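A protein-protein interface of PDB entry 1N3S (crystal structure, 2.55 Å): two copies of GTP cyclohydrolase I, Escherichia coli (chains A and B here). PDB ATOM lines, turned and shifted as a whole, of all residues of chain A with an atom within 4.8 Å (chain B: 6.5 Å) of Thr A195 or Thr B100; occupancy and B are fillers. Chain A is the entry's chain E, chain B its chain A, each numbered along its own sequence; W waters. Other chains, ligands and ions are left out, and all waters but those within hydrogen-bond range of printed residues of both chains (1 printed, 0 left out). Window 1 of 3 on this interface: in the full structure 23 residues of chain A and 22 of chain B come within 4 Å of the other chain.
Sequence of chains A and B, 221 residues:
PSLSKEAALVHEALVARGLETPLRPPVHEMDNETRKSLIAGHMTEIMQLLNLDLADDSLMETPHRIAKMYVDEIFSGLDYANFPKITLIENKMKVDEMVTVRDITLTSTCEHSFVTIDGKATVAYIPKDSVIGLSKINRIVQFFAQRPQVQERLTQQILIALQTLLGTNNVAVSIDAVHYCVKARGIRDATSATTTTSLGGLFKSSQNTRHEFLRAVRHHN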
ATOM      1  N   GLN A 151     -17.831 -25.608  21.351  1.00  0.00           N
ATOM      2  CA  GLN A 151     -18.125 -25.087  22.701  1.00  0.00           C
ATOM      3  C   GLN A 151     -18.045 -26.110  23.845  1.00  0.00           C
ATOM      4  O   GLN A 151     -17.453 -25.838  24.892  1.00  0.00           O
ATOM      5  CB  GLN A 151     -19.478 -24.340  22.734  1.00  0.00           C
ATOM      6  CG  GLN A 151     -19.512 -23.138  23.723  1.00  0.00           C
ATOM      7  CD  GLN A 151     -20.890 -22.481  23.871  1.00  0.00           C
ATOM      8  OE1 GLN A 151     -21.487 -22.040  22.894  1.00  0.00           O
ATOM      9  NE2 GLN A 151     -21.380 -22.392  25.105  1.00  0.00           N
ATOM     10  N   SER A 174     -18.084 -22.488  33.027  1.00  0.00           N
ATOM     11  CA  SER A 174     -19.305 -22.256  32.272  1.00  0.00           C
ATOM     12  C   SER A 174     -19.040 -21.203  31.221  1.00  0.00           C
ATOM     13  O   SER A 174     -18.454 -20.164  31.521  1.00  0.00           O
ATOM     14  CB  SER A 174     -20.428 -21.794  33.182  1.00  0.00           C
ATOM     15  OG  SER A 174     -21.654 -21.764  32.484  1.00  0.00           O
ATOM     16  N   ILE A 175     -19.415 -21.506  29.976  1.00  0.00           N
ATOM     17  CA  ILE A 175     -19.246 -20.576  28.859  1.00  0.00           C
ATOM     18  C   ILE A 175     -20.604 -20.271  28.240  1.00  0.00           C
ATOM     19  O   ILE A 175     -21.335 -21.184  27.857  1.00  0.00           O
ATOM     20  CB  ILE A 175     -18.264 -21.122  27.777  1.00  0.00           C
ATOM     21  CG1 ILE A 175     -16.874 -21.302  28.385  1.00  0.00           C
ATOM     22  CG2 ILE A 175     -18.152 -20.134  26.599  1.00  0.00           C
ATOM     23  CD1 ILE A 175     -15.928 -22.084  27.565  1.00  0.00           C
ATOM     24  N   ASP A 176     -20.938 -18.980  28.206  1.00  0.00           N
ATOM     25  CA  ASP A 176     -22.180 -18.467  27.631  1.00  0.00           C
ATOM     26  C   ASP A 176     -21.761 -17.830  26.302  1.00  0.00           C
ATOM     27  O   ASP A 176     -20.932 -16.911  26.278  1.00  0.00           O
ATOM     28  CB  ASP A 176     -22.812 -17.437  28.572  1.00  0.00           C
ATOM     29  CG  ASP A 176     -24.251 -17.128  28.218  1.00  0.00           C
ATOM     30  OD1 ASP A 176     -24.943 -18.015  27.664  1.00  0.00           O
ATOM     31  OD2 ASP A 176     -24.695 -15.991  28.497  1.00  0.00           O
ATOM     32  N   ALA A 193     -28.748 -18.001  22.635  1.00  0.00           N
ATOM     33  CA  ALA A 193     -27.384 -18.091  23.140  1.00  0.00           C
ATOM     34  C   ALA A 193     -27.258 -19.483  23.737  1.00  0.00           C
ATOM     35  O   ALA A 193     -28.258 -20.085  24.157  1.00  0.00           O
ATOM     36  CB  ALA A 193     -27.133 -17.035  24.210  1.00  0.00           C
ATOM     37  N   THR A 194     -26.030 -19.976  23.788  1.00  0.00           N
ATOM     38  CA  THR A 194     -25.747 -21.304  24.310  1.00  0.00           C
ATOM     39  C   THR A 194     -24.865 -21.250  25.549  1.00  0.00           C
ATOM     40  O   THR A 194     -23.829 -20.583  25.549  1.00  0.00           O
ATOM     41  CB  THR A 194     -25.032 -22.186  23.219  1.00  0.00           C
ATOM     42  OG1 THR A 194     -25.851 -22.251  22.045  1.00  0.00           O
ATOM     43  CG2 THR A 194     -24.752 -23.611  23.736  1.00  0.00           C
ATOM     44  N   THR A 195     -25.260 -22.011  26.570  1.00  0.00           N
ATOM     45  CA  THR A 195     -24.504 -22.113  27.820  1.00  0.00           C
ATOM     46  C   THR A 195     -24.044 -23.566  28.009  1.00  0.00           C
ATOM     47  O   THR A 195     -24.867 -24.480  28.069  1.00  0.00           O
ATOM     48  CB  THR A 195     -25.340 -21.670  29.056  1.00  0.00           C
ATOM     49  OG1 THR A 195     -25.860 -20.348  28.843  1.00  0.00           O
ATOM     50  CG2 THR A 195     -24.476 -21.648  30.300  1.00  0.00           C
ATOM     51  N   THR A 196     -22.729 -23.762  28.060  1.00  0.00           N
ATOM     52  CA  THR A 196     -22.127 -25.080  28.260  1.00  0.00           C
ATOM     53  C   THR A 196     -21.401 -25.051  29.607  1.00  0.00           C
ATOM     54  O   THR A 196     -20.496 -24.233  29.796  1.00  0.00           O
ATOM     55  CB  THR A 196     -21.109 -25.426  27.137  1.00  0.00           C
ATOM     56  OG1 THR A 196     -20.191 -24.339  26.953  1.00  0.00           O
ATOM     57  CG2 THR A 196     -21.817 -25.721  25.830  1.00  0.00           C
ATOM     58  N   THR A 197     -21.846 -25.888  30.553  1.00  0.00           N
ATOM     59  CA  THR A 197     -21.247 -25.945  31.893  1.00  0.00           C
ATOM     60  C   THR A 197     -20.602 -27.295  32.260  1.00  0.00           C
ATOM     61  O   THR A 197     -21.267 -28.325  32.251  1.00  0.00           O
ATOM     62  CB  THR A 197     -22.258 -25.518  33.061  1.00  0.00           C
ATOM     63  OG1 THR A 197     -22.958 -26.659  33.567  1.00  0.00           O
ATOM     64  CG2 THR A 197     -23.304 -24.515  32.594  1.00  0.00           C
ATOM     65  N   MET B  98     -23.459 -30.359  31.165  1.00  0.00           N
ATOM     66  CA  MET B  98     -24.762 -29.848  30.733  1.00  0.00           C
ATOM     67  C   MET B  98     -24.723 -28.708  29.691  1.00  0.00           C
ATOM     68  O   MET B  98     -23.894 -27.794  29.769  1.00  0.00           O
ATOM     69  CB  MET B  98     -25.616 -29.508  31.968  1.00  0.00           C
ATOM     70  CG  MET B  98     -26.448 -28.245  31.921  1.00  0.00           C
ATOM     71  SD  MET B  98     -27.785 -28.391  33.056  1.00  0.00           S
ATOM     72  CE  MET B  98     -28.980 -27.739  32.166  1.00  0.00           C
ATOM     73  N   VAL B  99     -25.574 -28.832  28.671  1.00  0.00           N
ATOM     74  CA  VAL B  99     -25.661 -27.828  27.610  1.00  0.00           C
ATOM     75  C   VAL B  99     -27.066 -27.259  27.645  1.00  0.00           C
ATOM     76  O   VAL B  99     -28.035 -28.017  27.679  1.00  0.00           O
ATOM     77  CB  VAL B  99     -25.393 -28.411  26.161  1.00  0.00           C
ATOM     78  CG1 VAL B  99     -25.232 -27.283  25.136  1.00  0.00           C
ATOM     79  CG2 VAL B  99     -24.169 -29.298  26.118  1.00  0.00           C
ATOM     80  N   THR B 100     -27.163 -25.928  27.657  1.00  0.00           N
ATOM     81  CA  THR B 100     -28.450 -25.228  27.684  1.00  0.00           C
ATOM     82  C   THR B 100     -28.492 -24.181  26.585  1.00  0.00           C
ATOM     83  O   THR B 100     -27.604 -23.343  26.501  1.00  0.00           O
ATOM     84  CB  THR B 100     -28.675 -24.500  29.044  1.00  0.00           C
ATOM     85  OG1 THR B 100     -28.372 -25.396  30.122  1.00  0.00           O
ATOM     86  CG2 THR B 100     -30.119 -24.013  29.194  1.00  0.00           C
ATOM     87  N   VAL B 101     -29.484 -24.272  25.705  1.00  0.00           N
ATOM     88  CA  VAL B 101     -29.659 -23.285  24.635  1.00  0.00           C
ATOM     89  C   VAL B 101     -30.948 -22.560  24.992  1.00  0.00           C
ATOM     90  O   VAL B 101     -32.037 -23.132  24.918  1.00  0.00           O
ATOM     91  CB  VAL B 101     -29.773 -23.918  23.223  1.00  0.00           C
ATOM     92  CG1 VAL B 101     -29.828 -22.821  22.163  1.00  0.00           C
ATOM     93  CG2 VAL B 101     -28.585 -24.823  22.945  1.00  0.00           C
ATOM     94  N   ARG B 102     -30.807 -21.314  25.434  1.00  0.00           N
ATOM     95  CA  ARG B 102     -31.956 -20.508  25.843  1.00  0.00           C
ATOM     96  C   ARG B 102     -32.302 -19.455  24.811  1.00  0.00           C
ATOM     97  O   ARG B 102     -31.526 -19.208  23.884  1.00  0.00           O
ATOM     98  CB  ARG B 102     -31.709 -19.842  27.213  1.00  0.00           C
ATOM     99  CG  ARG B 102     -30.751 -18.645  27.216  1.00  0.00           C
ATOM    100  CD  ARG B 102     -29.300 -19.032  27.527  1.00  0.00           C
ATOM    101  NE  ARG B 102     -28.319 -17.945  27.362  1.00  0.00           N
ATOM    102  CZ  ARG B 102     -28.417 -16.705  27.851  1.00  0.00           C
ATOM    103  NH1 ARG B 102     -29.467 -16.322  28.565  1.00  0.00           N
ATOM    104  NH2 ARG B 102     -27.442 -15.837  27.612  1.00  0.00           N
ATOM    105  N   THR B 122     -36.462 -22.795  25.735  1.00  0.00           N
ATOM    106  CA  THR B 122     -35.275 -23.099  26.501  1.00  0.00           C
ATOM    107  C   THR B 122     -35.187 -24.616  26.498  1.00  0.00           C
ATOM    108  O   THR B 122     -36.143 -25.314  26.864  1.00  0.00           O
ATOM    109  CB  THR B 122     -35.395 -22.526  27.943  1.00  0.00           C
ATOM    110  OG1 THR B 122     -35.739 -21.137  27.857  1.00  0.00           O
ATOM    111  CG2 THR B 122     -34.078 -22.650  28.691  1.00  0.00           C
ATOM    112  N   VAL B 123     -34.066 -25.106  25.980  1.00  0.00           N
ATOM    113  CA  VAL B 123     -33.788 -26.528  25.886  1.00  0.00           C
ATOM    114  C   VAL B 123     -32.465 -26.793  26.566  1.00  0.00           C
ATOM    115  O   VAL B 123     -31.470 -26.107  26.305  1.00  0.00           O
ATOM    116  CB  VAL B 123     -33.733 -27.009  24.383  1.00  0.00           C
ATOM    117  CG1 VAL B 123     -33.034 -28.380  24.238  1.00  0.00           C
ATOM    118  CG2 VAL B 123     -35.153 -27.104  23.806  1.00  0.00           C
ATOM    119  N   ALA B 124     -32.471 -27.804  27.429  1.00  0.00           N
ATOM    120  CA  ALA B 124     -31.278 -28.219  28.150  1.00  0.00           C
ATOM    121  C   ALA B 124     -31.173 -29.738  28.134  1.00  0.00           C
ATOM    122  O   ALA B 124     -32.198 -30.433  28.201  1.00  0.00           O
ATOM    123  CB  ALA B 124     -31.328 -27.714  29.562  1.00  0.00           C
ATOM    124  N   TYR B 125     -29.945 -30.239  27.988  1.00  0.00           N
ATOM    125  CA  TYR B 125     -29.688 -31.679  27.968  1.00  0.00           C
ATOM    126  C   TYR B 125     -28.301 -32.067  28.484  1.00  0.00           C
ATOM    127  O   TYR B 125     -27.366 -31.250  28.480  1.00  0.00           O
ATOM    128  CB  TYR B 125     -29.922 -32.273  26.555  1.00  0.00           C
ATOM    129  CG  TYR B 125     -28.813 -32.059  25.534  1.00  0.00           C
ATOM    130  CD1 TYR B 125     -28.586 -30.788  24.957  1.00  0.00           C
ATOM    131  CD2 TYR B 125     -27.970 -33.126  25.155  1.00  0.00           C
ATOM    132  CE1 TYR B 125     -27.532 -30.585  24.020  1.00  0.00           C
ATOM    133  CE2 TYR B 125     -26.919 -32.937  24.222  1.00  0.00           C
ATOM    134  CZ  TYR B 125     -26.701 -31.666  23.664  1.00  0.00           C
ATOM    135  OH  TYR B 125     -25.660 -31.480  22.776  1.00  0.00           O
ATOM    136  N   PHE B 203     -33.605 -34.388  35.051  1.00  0.00           N
ATOM    137  CA  PHE B 203     -34.323 -33.124  35.242  1.00  0.00           C
ATOM    138  C   PHE B 203     -35.705 -33.357  35.863  1.00  0.00           C
ATOM    139  O   PHE B 203     -36.363 -32.414  36.288  1.00  0.00           O
ATOM    140  CB  PHE B 203     -34.513 -32.404  33.899  1.00  0.00           C
ATOM    141  CG  PHE B 203     -33.234 -31.964  33.248  1.00  0.00           C
ATOM    142  CD1 PHE B 203     -32.632 -30.751  33.605  1.00  0.00           C
ATOM    143  CD2 PHE B 203     -32.642 -32.740  32.239  1.00  0.00           C
ATOM    144  CE1 PHE B 203     -31.445 -30.297  32.961  1.00  0.00           C
ATOM    145  CE2 PHE B 203     -31.450 -32.304  31.579  1.00  0.00           C
ATOM    146  CZ  PHE B 203     -30.851 -31.078  31.942  1.00  0.00           C
ATOM    147  N   GLU B 212     -31.713 -27.314  38.645  1.00  0.00           N
ATOM    148  CA  GLU B 212     -30.557 -26.813  37.885  1.00  0.00           C
ATOM    149  C   GLU B 212     -31.022 -26.114  36.609  1.00  0.00           C
ATOM    150  O   GLU B 212     -30.404 -25.158  36.136  1.00  0.00           O
ATOM    151  CB  GLU B 212     -29.577 -27.930  37.501  1.00  0.00           C
ATOM    152  CG  GLU B 212     -28.599 -28.347  38.593  1.00  0.00           C
ATOM    153  CD  GLU B 212     -27.556 -29.341  38.099  1.00  0.00           C
ATOM    154  OE1 GLU B 212     -26.750 -28.975  37.215  1.00  0.00           O
ATOM    155  OE2 GLU B 212     -27.544 -30.487  38.594  1.00  0.00           O
ATOM    156  N   PHE B 213     -32.119 -26.613  36.058  1.00  0.00           N
ATOM    157  CA  PHE B 213     -32.702 -26.063  34.847  1.00  0.00           C
ATOM    158  C   PHE B 213     -33.683 -24.954  35.194  1.00  0.00           C
ATOM    159  O   PHE B 213     -33.540 -23.826  34.729  1.00  0.00           O
ATOM    160  CB  PHE B 213     -33.419 -27.181  34.079  1.00  0.00           C
ATOM    161  CG  PHE B 213     -34.259 -26.708  32.924  1.00  0.00           C
ATOM    162  CD1 PHE B 213     -33.660 -26.188  31.767  1.00  0.00           C
ATOM    163  CD2 PHE B 213     -35.660 -26.813  32.980  1.00  0.00           C
ATOM    164  CE1 PHE B 213     -34.443 -25.780  30.670  1.00  0.00           C
ATOM    165  CE2 PHE B 213     -36.461 -26.410  31.892  1.00  0.00           C
ATOM    166  CZ  PHE B 213     -35.845 -25.892  30.730  1.00  0.00           C
ATOM    167  N   ALA B 216     -32.467 -21.516  35.910  1.00  0.00           N
ATOM    168  CA  ALA B 216     -31.880 -20.906  34.719  1.00  0.00           C
ATOM    169  C   ALA B 216     -32.945 -20.737  33.610  1.00  0.00           C
ATOM    170  O   ALA B 216     -32.617 -20.563  32.427  1.00  0.00           O
ATOM    171  CB  ALA B 216     -30.685 -21.764  34.231  1.00  0.00           C
HETATM  172  O   HOH W   1     -25.711 -24.995  30.413  1.00  0.00           O
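No position is printed for both chains. Of the 13 pairs that touch across the chains among the printed residues, none has its exchanged pair printed and touching as well.
Of the 13 printed residues of chain B, 5 touch a printed residue of chain A. Of the 9 printed residues of chain A, 6 touch a printed residue of chain B. Hydrophobic or aromatic side chains of chain A within 4 Å of the printed part of chain B: Ala A193. Among the printed residues, Asp or Glu carboxylates within 4 Å of a Lys or Arg side-chain nitrogen of the other chain: Asp A176 with Arg B102.
Water W1 lies within hydrogen-bond range of the backbone carbonyl oxygen (O) of Thr A195 (2.5 Å), the side-chain hydroxyl (OG1) of Thr B100 (2.7 Å) and the backbone carbonyl oxygen (O) of Met B98 (3.4 Å).
O of Met B98 lies within hydrogen-bond range of N of Thr A197 (2.9 Å). The guanidinium group (NH2) of Arg B102 is in salt-bridge range of the side-chain carboxylate (OD2) of Asp A176. The backbone carbonyl oxygen (O) of Ala A193 lies within hydrogen-bond range of the backbone NH (N) of Arg B102 (3.1 Å). The backbone carbonyl oxygen (O) of Thr B100 is in hydrogen-bond range of the backbone NH (N) of Thr A195 (2.7 Å).
The backbone NH of Thr A196 is in hydrogen-bond range of the backbone carbonyl oxygen of Ile A175. The side-chain hydroxyl of Thr A195 lies within hydrogen-bond range of the side-chain carboxylate of Asp A176 (2.8 Å). N of Tyr B125 is in hydrogen-bond range of O of Val B99. The backbone carbonyl oxygen (O) of Thr A194 lies within hydrogen-bond range of the side-chain amide nitrogen (NE2) of Gln A151. The side-chain hydroxyl of Thr A196 lies within hydrogen-bond range of the side-chain amide nitrogen of Gln A151 (2.9 Å). The backbone carbonyl oxygen (O) of Val B123 lies within hydrogen-bond range of the backbone NH (N) of Val B101 (2.8 Å).
Ser A174 touches none of the printed residues of chain B. Of the printed residues of chain B, Asp A176 touches Arg B102 (2.9 Å). Printed residues of chain B within 4 Å of Ala A193: Val B101 (3.5 Å) and Arg B102 (3.1 Å). Of the printed residues of chain B, Thr A194 touches Val B99 (3.96 Å), Thr B100 (3.5 Å) and Val B101 (3.9 Å). Thr A195 touches four residues of chain B. Printed residues of chain B within 4 Å of Thr A197: Met B98 (2.9 Å). Of chain A, only Thr A194 and Thr A195 come within 4 Å of Thr B100. Thr B122 touches none of the printed residues of chain A.
Among the printed residues, merely in contact across the chains: Ala A193 with Val B101 (3.5 Å), Thr A194 with Val B99 (3.96 Å), Thr A194 with Thr B100 (3.5 Å), Thr A194 with Val B101 (3.9 Å), Thr A195 with Met B98 (3.8 Å), Thr A195 with Val B99 (3.5 Å), Thr A195 with Arg B102 (3.7 Å), Thr A196 with Met B98 (3.6 Å) and Thr A196 with Val B99 (3.8 Å).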
